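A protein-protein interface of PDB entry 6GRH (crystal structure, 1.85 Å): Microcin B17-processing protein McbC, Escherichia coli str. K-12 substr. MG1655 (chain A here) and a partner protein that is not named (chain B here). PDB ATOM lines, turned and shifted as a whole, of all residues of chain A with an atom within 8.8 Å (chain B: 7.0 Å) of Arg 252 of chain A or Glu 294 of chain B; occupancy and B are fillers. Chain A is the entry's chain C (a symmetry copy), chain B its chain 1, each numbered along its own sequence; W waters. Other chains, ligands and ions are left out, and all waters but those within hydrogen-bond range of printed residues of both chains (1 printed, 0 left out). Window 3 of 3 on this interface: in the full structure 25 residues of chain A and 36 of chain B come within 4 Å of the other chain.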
ATOM      1  N   LEU A  20     -33.434  -9.131  20.784  1.00  0.00           N
ATOM      2  CA  LEU A  20     -32.502  -9.872  19.958  1.00  0.00           C
ATOM      3  C   LEU A  20     -33.047 -10.151  18.559  1.00  0.00           C
ATOM      4  O   LEU A  20     -32.341  -9.926  17.578  1.00  0.00           O
ATOM      5  CB  LEU A  20     -32.098 -11.157  20.636  1.00  0.00           C
ATOM      6  CG  LEU A  20     -31.103 -12.033  19.899  1.00  0.00           C
ATOM      7  CD1 LEU A  20     -29.799 -11.273  19.721  1.00  0.00           C
ATOM      8  CD2 LEU A  20     -30.884 -13.297  20.716  1.00  0.00           C
ATOM      9  N   ALA A  21     -34.276 -10.643  18.479  1.00  0.00           N
ATOM     10  CA  ALA A  21     -34.900 -10.975  17.196  1.00  0.00           C
ATOM     11  C   ALA A  21     -35.106  -9.754  16.328  1.00  0.00           C
ATOM     12  O   ALA A  21     -34.804  -9.792  15.149  1.00  0.00           O
ATOM     13  CB  ALA A  21     -36.234 -11.689  17.408  1.00  0.00           C
ATOM     14  N   LYS A  24     -31.680  -8.624  15.016  1.00  0.00           N
ATOM     15  CA  LYS A  24     -31.199  -9.490  13.944  1.00  0.00           C
ATOM     16  C   LYS A  24     -31.969  -9.312  12.637  1.00  0.00           C
ATOM     17  O   LYS A  24     -31.372  -9.324  11.550  1.00  0.00           O
ATOM     18  CB  LYS A  24     -31.253 -10.949  14.362  1.00  0.00           C
ATOM     19  CG  LYS A  24     -30.223 -11.388  15.388  1.00  0.00           C
ATOM     20  CD  LYS A  24     -30.656 -12.801  15.814  1.00  0.00           C
ATOM     21  CE  LYS A  24     -29.572 -13.582  16.449  1.00  0.00           C
ATOM     22  NZ  LYS A  24     -30.017 -15.008  16.652  1.00  0.00           N
ATOM     23  N   ILE A 193     -19.629  -8.273  15.475  1.00  0.00           N
ATOM     24  CA  ILE A 193     -20.493  -7.991  16.600  1.00  0.00           C
ATOM     25  C   ILE A 193     -21.013  -9.297  17.211  1.00  0.00           C
ATOM     26  O   ILE A 193     -21.524 -10.157  16.494  1.00  0.00           O
ATOM     27  CB  ILE A 193     -21.693  -7.103  16.207  1.00  0.00           C
ATOM     28  CG1 ILE A 193     -22.495  -6.704  17.461  1.00  0.00           C
ATOM     29  CG2 ILE A 193     -22.609  -7.745  15.169  1.00  0.00           C
ATOM     30  CD1 ILE A 193     -23.587  -5.715  17.152  1.00  0.00           C
ATOM     31  N   ILE A 194     -20.899  -9.425  18.528  1.00  0.00           N
ATOM     32  CA  ILE A 194     -21.591 -10.484  19.257  1.00  0.00           C
ATOM     33  C   ILE A 194     -22.928  -9.898  19.697  1.00  0.00           C
ATOM     34  O   ILE A 194     -22.959  -9.058  20.596  1.00  0.00           O
ATOM     35  CB  ILE A 194     -20.773 -10.962  20.472  1.00  0.00           C
ATOM     36  CG1 ILE A 194     -19.425 -11.488  19.995  1.00  0.00           C
ATOM     37  CG2 ILE A 194     -21.556 -12.038  21.244  1.00  0.00           C
ATOM     38  CD1 ILE A 194     -18.539 -11.931  21.124  1.00  0.00           C
ATOM     39  N   PHE A 195     -24.020 -10.344  19.104  1.00  0.00           N
ATOM     40  CA  PHE A 195     -25.316  -9.649  19.292  1.00  0.00           C
ATOM     41  C   PHE A 195     -25.708  -9.528  20.745  1.00  0.00           C
ATOM     42  O   PHE A 195     -26.045  -8.442  21.220  1.00  0.00           O
ATOM     43  CB  PHE A 195     -26.446 -10.310  18.525  1.00  0.00           C
ATOM     44  CG  PHE A 195     -26.312 -10.186  17.029  1.00  0.00           C
ATOM     45  CD1 PHE A 195     -26.534  -8.978  16.399  1.00  0.00           C
ATOM     46  CD2 PHE A 195     -25.947 -11.285  16.261  1.00  0.00           C
ATOM     47  CE1 PHE A 195     -26.426  -8.865  15.015  1.00  0.00           C
ATOM     48  CE2 PHE A 195     -25.836 -11.178  14.873  1.00  0.00           C
ATOM     49  CZ  PHE A 195     -26.074  -9.958  14.258  1.00  0.00           C
ATOM     50  N   GLU A 196     -25.645 -10.642  21.457  1.00  0.00           N
ATOM     51  CA  GLU A 196     -26.123 -10.639  22.834  1.00  0.00           C
ATOM     52  C   GLU A 196     -25.254  -9.810  23.765  1.00  0.00           C
ATOM     53  O   GLU A 196     -25.786  -9.211  24.685  1.00  0.00           O
ATOM     54  CB  GLU A 196     -26.332 -12.070  23.339  1.00  0.00           C
ATOM     55  CG  GLU A 196     -27.559 -12.697  22.668  1.00  0.00           C
ATOM     56  CD  GLU A 196     -28.017 -14.006  23.288  1.00  0.00           C
ATOM     57  OE1 GLU A 196     -28.191 -14.066  24.534  1.00  0.00           O
ATOM     58  OE2 GLU A 196     -28.266 -14.956  22.516  1.00  0.00           O
ATOM     59  N   ALA A 244     -18.769 -15.220   7.186  1.00  0.00           N
ATOM     60  CA  ALA A 244     -19.026 -15.895   8.461  1.00  0.00           C
ATOM     61  C   ALA A 244     -18.774 -17.415   8.389  1.00  0.00           C
ATOM     62  O   ALA A 244     -18.080 -17.968   9.234  1.00  0.00           O
ATOM     63  CB  ALA A 244     -20.424 -15.598   8.978  1.00  0.00           C
ATOM     64  N   LYS A 245     -19.322 -18.064   7.361  1.00  0.00           N
ATOM     65  CA  LYS A 245     -19.215 -19.510   7.173  1.00  0.00           C
ATOM     66  C   LYS A 245     -17.741 -19.924   7.006  1.00  0.00           C
ATOM     67  O   LYS A 245     -17.273 -20.902   7.631  1.00  0.00           O
ATOM     68  CB  LYS A 245     -20.015 -19.916   5.939  1.00  0.00           C
ATOM     69  CG  LYS A 245     -19.950 -21.384   5.506  1.00  0.00           C
ATOM     70  CD  LYS A 245     -20.895 -22.245   6.335  1.00  0.00           C
ATOM     71  CE  LYS A 245     -20.806 -23.718   5.912  1.00  0.00           C
ATOM     72  NZ  LYS A 245     -22.164 -24.343   5.827  1.00  0.00           N
ATOM     73  N   ASN A 248     -15.866 -19.997  10.059  1.00  0.00           N
ATOM     74  CA  ASN A 248     -16.547 -20.871  11.000  1.00  0.00           C
ATOM     75  C   ASN A 248     -17.239 -20.111  12.149  1.00  0.00           C
ATOM     76  O   ASN A 248     -17.346 -20.615  13.264  1.00  0.00           O
ATOM     77  CB  ASN A 248     -15.595 -21.960  11.520  1.00  0.00           C
ATOM     78  CG  ASN A 248     -15.271 -22.986  10.456  1.00  0.00           C
ATOM     79  OD1 ASN A 248     -16.159 -23.437   9.737  1.00  0.00           O
ATOM     80  ND2 ASN A 248     -14.019 -23.347  10.349  1.00  0.00           N
ATOM     81  N   LEU A 249     -17.742 -18.919  11.858  1.00  0.00           N
ATOM     82  CA  LEU A 249     -18.519 -18.176  12.846  1.00  0.00           C
ATOM     83  C   LEU A 249     -19.962 -18.686  12.851  1.00  0.00           C
ATOM     84  O   LEU A 249     -20.510 -19.017  11.791  1.00  0.00           O
ATOM     85  CB  LEU A 249     -18.523 -16.690  12.533  1.00  0.00           C
ATOM     86  CG  LEU A 249     -17.197 -15.926  12.492  1.00  0.00           C
ATOM     87  CD1 LEU A 249     -17.485 -14.456  12.201  1.00  0.00           C
ATOM     88  CD2 LEU A 249     -16.449 -16.057  13.777  1.00  0.00           C
ATOM     89  N   ASP A 250     -20.594 -18.676  14.021  1.00  0.00           N
ATOM     90  CA  ASP A 250     -22.011 -19.010  14.161  1.00  0.00           C
ATOM     91  C   ASP A 250     -22.849 -17.729  14.055  1.00  0.00           C
ATOM     92  O   ASP A 250     -22.888 -16.902  14.993  1.00  0.00           O
ATOM     93  CB  ASP A 250     -22.260 -19.702  15.487  1.00  0.00           C
ATOM     94  CG  ASP A 250     -23.676 -20.345  15.586  1.00  0.00           C
ATOM     95  OD1 ASP A 250     -24.678 -19.870  14.982  1.00  0.00           O
ATOM     96  OD2 ASP A 250     -23.785 -21.360  16.320  1.00  0.00           O
ATOM     97  N   GLN A 251     -23.523 -17.592  12.906  1.00  0.00           N
ATOM     98  CA  GLN A 251     -24.311 -16.397  12.581  1.00  0.00           C
ATOM     99  C   GLN A 251     -25.484 -16.121  13.485  1.00  0.00           C
ATOM    100  O   GLN A 251     -25.982 -15.011  13.475  1.00  0.00           O
ATOM    101  CB  GLN A 251     -24.800 -16.456  11.136  1.00  0.00           C
ATOM    102  CG  GLN A 251     -23.689 -16.185  10.132  1.00  0.00           C
ATOM    103  CD  GLN A 251     -24.166 -16.461   8.731  1.00  0.00           C
ATOM    104  OE1 GLN A 251     -24.849 -15.627   8.169  1.00  0.00           O
ATOM    105  NE2 GLN A 251     -23.893 -17.659   8.204  1.00  0.00           N
ATOM    106  N   ARG A 252     -25.930 -17.110  14.268  1.00  0.00           N
ATOM    107  CA  ARG A 252     -26.907 -16.853  15.347  1.00  0.00           C
ATOM    108  C   ARG A 252     -26.346 -16.001  16.486  1.00  0.00           C
ATOM    109  O   ARG A 252     -27.114 -15.338  17.197  1.00  0.00           O
ATOM    110  CB  ARG A 252     -27.452 -18.156  15.920  1.00  0.00           C
ATOM    111  CG  ARG A 252     -28.263 -18.974  14.929  1.00  0.00           C
ATOM    112  CD  ARG A 252     -28.497 -20.406  15.410  1.00  0.00           C
ATOM    113  NE  ARG A 252     -27.248 -21.145  15.590  1.00  0.00           N
ATOM    114  CZ  ARG A 252     -27.162 -22.421  15.957  1.00  0.00           C
ATOM    115  NH1 ARG A 252     -28.247 -23.150  16.183  1.00  0.00           N
ATOM    116  NH2 ARG A 252     -25.968 -22.991  16.088  1.00  0.00           N
ATOM    117  N   THR A 253     -25.028 -16.000  16.654  1.00  0.00           N
ATOM    118  CA  THR A 253     -24.380 -15.295  17.752  1.00  0.00           C
ATOM    119  C   THR A 253     -23.605 -14.082  17.305  1.00  0.00           C
ATOM    120  O   THR A 253     -23.598 -13.068  18.018  1.00  0.00           O
ATOM    121  CB  THR A 253     -23.435 -16.279  18.466  1.00  0.00           C
ATOM    122  OG1 THR A 253     -24.226 -17.271  19.106  1.00  0.00           O
ATOM    123  CG2 THR A 253     -22.566 -15.621  19.514  1.00  0.00           C
ATOM    124  N   VAL A 254     -22.917 -14.201  16.157  1.00  0.00           N
ATOM    125  CA  VAL A 254     -21.891 -13.243  15.742  1.00  0.00           C
ATOM    126  C   VAL A 254     -21.954 -12.982  14.223  1.00  0.00           C
ATOM    127  O   VAL A 254     -22.250 -13.892  13.430  1.00  0.00           O
ATOM    128  CB  VAL A 254     -20.484 -13.671  16.248  1.00  0.00           C
ATOM    129  CG1 VAL A 254     -20.092 -15.064  15.784  1.00  0.00           C
ATOM    130  CG2 VAL A 254     -19.399 -12.683  15.862  1.00  0.00           C
ATOM    131  N   ALA A 255     -21.780 -11.719  13.831  1.00  0.00           N
ATOM    132  CA  ALA A 255     -21.896 -11.306  12.426  1.00  0.00           C
ATOM    133  C   ALA A 255     -20.734 -10.352  12.096  1.00  0.00           C
ATOM    134  O   ALA A 255     -20.398  -9.518  12.901  1.00  0.00           O
ATOM    135  CB  ALA A 255     -23.259 -10.655  12.141  1.00  0.00           C
ATOM    136  N   HIS B 286     -31.388 -16.698  10.406  1.00  0.00           N
ATOM    137  CA  HIS B 286     -31.273 -18.105  10.835  1.00  0.00           C
ATOM    138  C   HIS B 286     -32.135 -18.307  12.079  1.00  0.00           C
ATOM    139  O   HIS B 286     -32.145 -17.466  12.978  1.00  0.00           O
ATOM    140  CB  HIS B 286     -29.829 -18.454  11.176  1.00  0.00           C
ATOM    141  CG  HIS B 286     -28.923 -18.498   9.995  1.00  0.00           C
ATOM    142  ND1 HIS B 286     -28.248 -17.391   9.532  1.00  0.00           N
ATOM    143  CD2 HIS B 286     -28.569 -19.525   9.186  1.00  0.00           C
ATOM    144  CE1 HIS B 286     -27.524 -17.736   8.478  1.00  0.00           C
ATOM    145  NE2 HIS B 286     -27.693 -19.027   8.255  1.00  0.00           N
ATOM    146  N   TRP B 287     -32.918 -19.372  12.094  1.00  0.00           N
ATOM    147  CA  TRP B 287     -33.749 -19.651  13.246  1.00  0.00           C
ATOM    148  C   TRP B 287     -32.842 -20.202  14.355  1.00  0.00           C
ATOM    149  O   TRP B 287     -31.975 -21.056  14.110  1.00  0.00           O
ATOM    150  CB  TRP B 287     -34.840 -20.626  12.880  1.00  0.00           C
ATOM    151  CG  TRP B 287     -35.718 -21.022  13.995  1.00  0.00           C
ATOM    152  CD1 TRP B 287     -36.263 -20.221  14.943  1.00  0.00           C
ATOM    153  CD2 TRP B 287     -36.221 -22.333  14.232  1.00  0.00           C
ATOM    154  NE1 TRP B 287     -37.077 -20.949  15.759  1.00  0.00           N
ATOM    155  CE2 TRP B 287     -37.075 -22.254  15.337  1.00  0.00           C
ATOM    156  CE3 TRP B 287     -36.042 -23.569  13.593  1.00  0.00           C
ATOM    157  CZ2 TRP B 287     -37.750 -23.369  15.843  1.00  0.00           C
ATOM    158  CZ3 TRP B 287     -36.709 -24.686  14.095  1.00  0.00           C
ATOM    159  CH2 TRP B 287     -37.556 -24.572  15.210  1.00  0.00           C
ATOM    160  N   GLN B 288     -33.003 -19.660  15.553  1.00  0.00           N
ATOM    161  CA  GLN B 288     -32.165 -20.045  16.685  1.00  0.00           C
ATOM    162  C   GLN B 288     -32.107 -21.554  16.954  1.00  0.00           C
ATOM    163  O   GLN B 288     -31.059 -22.043  17.406  1.00  0.00           O
ATOM    164  CB  GLN B 288     -32.592 -19.306  17.967  1.00  0.00           C
ATOM    165  CG  GLN B 288     -34.029 -19.560  18.406  1.00  0.00           C
ATOM    166  CD  GLN B 288     -34.469 -18.592  19.475  1.00  0.00           C
ATOM    167  OE1 GLN B 288     -33.651 -18.099  20.272  1.00  0.00           O
ATOM    168  NE2 GLN B 288     -35.758 -18.275  19.485  1.00  0.00           N
ATOM    169  N   ALA B 289     -33.230 -22.263  16.736  1.00  0.00           N
ATOM    170  CA  ALA B 289     -33.282 -23.696  16.970  1.00  0.00           C
ATOM    171  C   ALA B 289     -32.945 -24.565  15.765  1.00  0.00           C
ATOM    172  O   ALA B 289     -33.060 -25.782  15.873  1.00  0.00           O
ATOM    173  CB  ALA B 289     -34.627 -24.117  17.517  1.00  0.00           C
ATOM    174  N   CYS B 290     -32.538 -23.969  14.651  1.00  0.00           N
ATOM    175  CA  CYS B 290     -32.201 -24.729  13.449  1.00  0.00           C
ATOM    176  C   CYS B 290     -30.749 -25.157  13.470  1.00  0.00           C
ATOM    177  O   CYS B 290     -29.897 -24.406  13.877  1.00  0.00           O
ATOM    178  CB  CYS B 290     -32.430 -23.894  12.198  1.00  0.00           C
ATOM    179  SG  CYS B 290     -32.419 -24.893  10.694  1.00  0.00           S
ATOM    180  N   SER B 291     -30.464 -26.330  12.943  1.00  0.00           N
ATOM    181  CA  SER B 291     -29.082 -26.824  12.865  1.00  0.00           C
ATOM    182  C   SER B 291     -28.423 -26.669  11.477  1.00  0.00           C
ATOM    183  O   SER B 291     -27.315 -27.183  11.286  1.00  0.00           O
ATOM    184  CB  SER B 291     -29.106 -28.294  13.239  1.00  0.00           C
ATOM    185  OG  SER B 291     -30.024 -28.922  12.348  1.00  0.00           O
ATOM    186  N   CYS B 292     -29.039 -25.936  10.540  1.00  0.00           N
ATOM    187  CA  CYS B 292     -28.443 -25.798   9.196  1.00  0.00           C
ATOM    188  C   CYS B 292     -27.025 -25.206   9.212  1.00  0.00           C
ATOM    189  O   CYS B 292     -26.156 -25.632   8.474  1.00  0.00           O
ATOM    190  CB  CYS B 292     -29.339 -25.027   8.216  1.00  0.00           C
ATOM    191  SG  CYS B 292     -29.791 -23.332   8.656  1.00  0.00           S
ATOM    192  N   LEU B 293     -26.805 -24.237  10.096  1.00  0.00           N
ATOM    193  CA  LEU B 293     -25.502 -23.598  10.277  1.00  0.00           C
ATOM    194  C   LEU B 293     -24.402 -24.531  10.755  1.00  0.00           C
ATOM    195  O   LEU B 293     -23.224 -24.299  10.481  1.00  0.00           O
ATOM    196  CB  LEU B 293     -25.625 -22.505  11.335  1.00  0.00           C
ATOM    197  CG  LEU B 293     -26.274 -21.253  10.803  1.00  0.00           C
ATOM    198  CD1 LEU B 293     -26.487 -20.284  11.941  1.00  0.00           C
ATOM    199  CD2 LEU B 293     -25.390 -20.680   9.710  1.00  0.00           C
ATOM    200  N   GLU B 294     -24.798 -25.544  11.516  1.00  0.00           N
ATOM    201  CA  GLU B 294     -23.858 -26.461  12.141  1.00  0.00           C
ATOM    202  C   GLU B 294     -23.431 -27.580  11.191  1.00  0.00           C
ATOM    203  O   GLU B 294     -22.430 -28.224  11.447  1.00  0.00           O
ATOM    204  CB  GLU B 294     -24.466 -27.049  13.409  1.00  0.00           C
ATOM    205  CG  GLU B 294     -24.947 -25.967  14.366  1.00  0.00           C
ATOM    206  CD  GLU B 294     -25.439 -26.496  15.710  1.00  0.00           C
ATOM    207  OE1 GLU B 294     -25.973 -27.636  15.786  1.00  0.00           O
ATOM    208  OE2 GLU B 294     -25.267 -25.742  16.713  1.00  0.00           O
ATOM    209  N   ARG B 295     -24.183 -27.811  10.118  1.00  0.00           N
ATOM    210  CA  ARG B 295     -23.871 -28.909   9.199  1.00  0.00           C
ATOM    211  C   ARG B 295     -22.685 -28.593   8.282  1.00  0.00           C
ATOM    212  O   ARG B 295     -22.347 -27.442   8.010  1.00  0.00           O
ATOM    213  CB  ARG B 295     -25.123 -29.341   8.411  1.00  0.00           C
ATOM    214  CG  ARG B 295     -26.142 -30.013   9.333  1.00  0.00           C
ATOM    215  CD  ARG B 295     -27.081 -30.972   8.627  1.00  0.00           C
ATOM    216  NE  ARG B 295     -28.021 -30.227   7.809  1.00  0.00           N
ATOM    217  CZ  ARG B 295     -29.123 -29.599   8.250  1.00  0.00           C
ATOM    218  NH1 ARG B 295     -29.450 -29.594   9.540  1.00  0.00           N
ATOM    219  NH2 ARG B 295     -29.906 -28.954   7.379  1.00  0.00           N
ATOM    220  OXT ARG B 295     -21.990 -29.508   7.820  1.00  0.00           O
HETATM  221  O   HOH W   1     -30.046 -15.901  13.974  1.00  0.00           O
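Leu 293 of chain B touches Asp 250 of chain A (CD1 to OD1, 3.6 Å). His 286 of chain B touches Gln 251 of chain A (CE1 to OE1, 3.4 Å). Gln 251 of chain A touches Leu 293 of chain B (NE2 to CD2, 3.7 Å). O of Trp 287 of chain B touches CD of Arg 252 of chain A (3.8 Å). CD1 of Leu 293 of chain B touches CG of Arg 252 of chain A, 3.7 Å away.
The backbone carbonyl oxygen (O) of Gln 288 of chain B sits at hydrogen-bond distance from the guanidinium group (NH1) of Arg 252 of chain A (3.3 Å). The guanidinium group (NH1) of Arg 252 of chain A is in hydrogen-bond range of the backbone carbonyl oxygen (O) of Cys 290 of chain B (3.1 Å). NH2 of Arg 252 of chain A is in salt-bridge range of OE2 of Glu 294 of chain B, at 2.9 Å. The side-chain amino group (NZ) of Lys 245 of chain A lies within salt-bridge range of the chain-end carboxylate (O) of Arg 295 of chain B (3.8 Å).
Printed residues of chain B within 4 Å of Arg 252 of chain A: Trp 287, Gln 288, Cys 290, Leu 293 and Glu 294. Glu 294 of chain B touches just one residue of chain A: Arg 252 (2.9 Å). Of the printed residues of chain A, Leu 293 of chain B touches Asp 250, Gln 251 and Arg 252. Printed residues of chain A within 4 Å of Cys 290 of chain B: Arg 252 (3.1 Å). Printed residues of chain A within 4 Å of Arg 295 of chain B: Lys 245. Of the printed residues of chain A, Trp 287 of chain B touches Arg 252. Of the printed residues of chain B, Lys 245 of chain A touches Arg 295. The nearest printed residue of chain B that does not touch Arg 252 of chain A is His 286 of chain B (4.1 Å). The nearest residue of chain A that does not touch Glu 294 of chain B is Asp 250 of chain A (4.6 Å). The nearest printed residue of chain A that does not touch Gln 288 of chain B is Lys 24 of chain A (5.2 Å).
Water W1 bridges the backbone carbonyl oxygen of His 286 of chain B (2.8 Å) and the side-chain amino group of Lys 24 of chain A (2.8 Å).
Printed residues of chain A that touch a printed residue of chain B: Lys 245, Asp 250, Gln 251 and Arg 252. Along chain A the printed residues that touch a printed residue of chain B span positions 245 to 252. Of the 10 printed residues of chain B, 7 touch a printed residue of chain A. Hydrophobic or aromatic side chains of chain B within 4 Å of the printed part of chain A: His 286 and Leu 293.
The side-chain hydroxyl (OG) of Ser 291 of chain B is in hydrogen-bond range of the guanidinium group (NH1) of Arg 295 of chain B. The side-chain amino group (NZ) of Lys 24 of chain A lies within hydrogen-bond range of the backbone carbonyl oxygen (O) of Arg 252 of chain A, at 3.0 Å. The backbone carbonyl oxygen of Lys 245 of chain A lies close to the side-chain amide oxygen of Asn 248 of chain A (3.5 Å). OD2 of Asp 250 of chain A is in salt-bridge range of NH2 of Arg 252 of chain A (2.7 Å).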
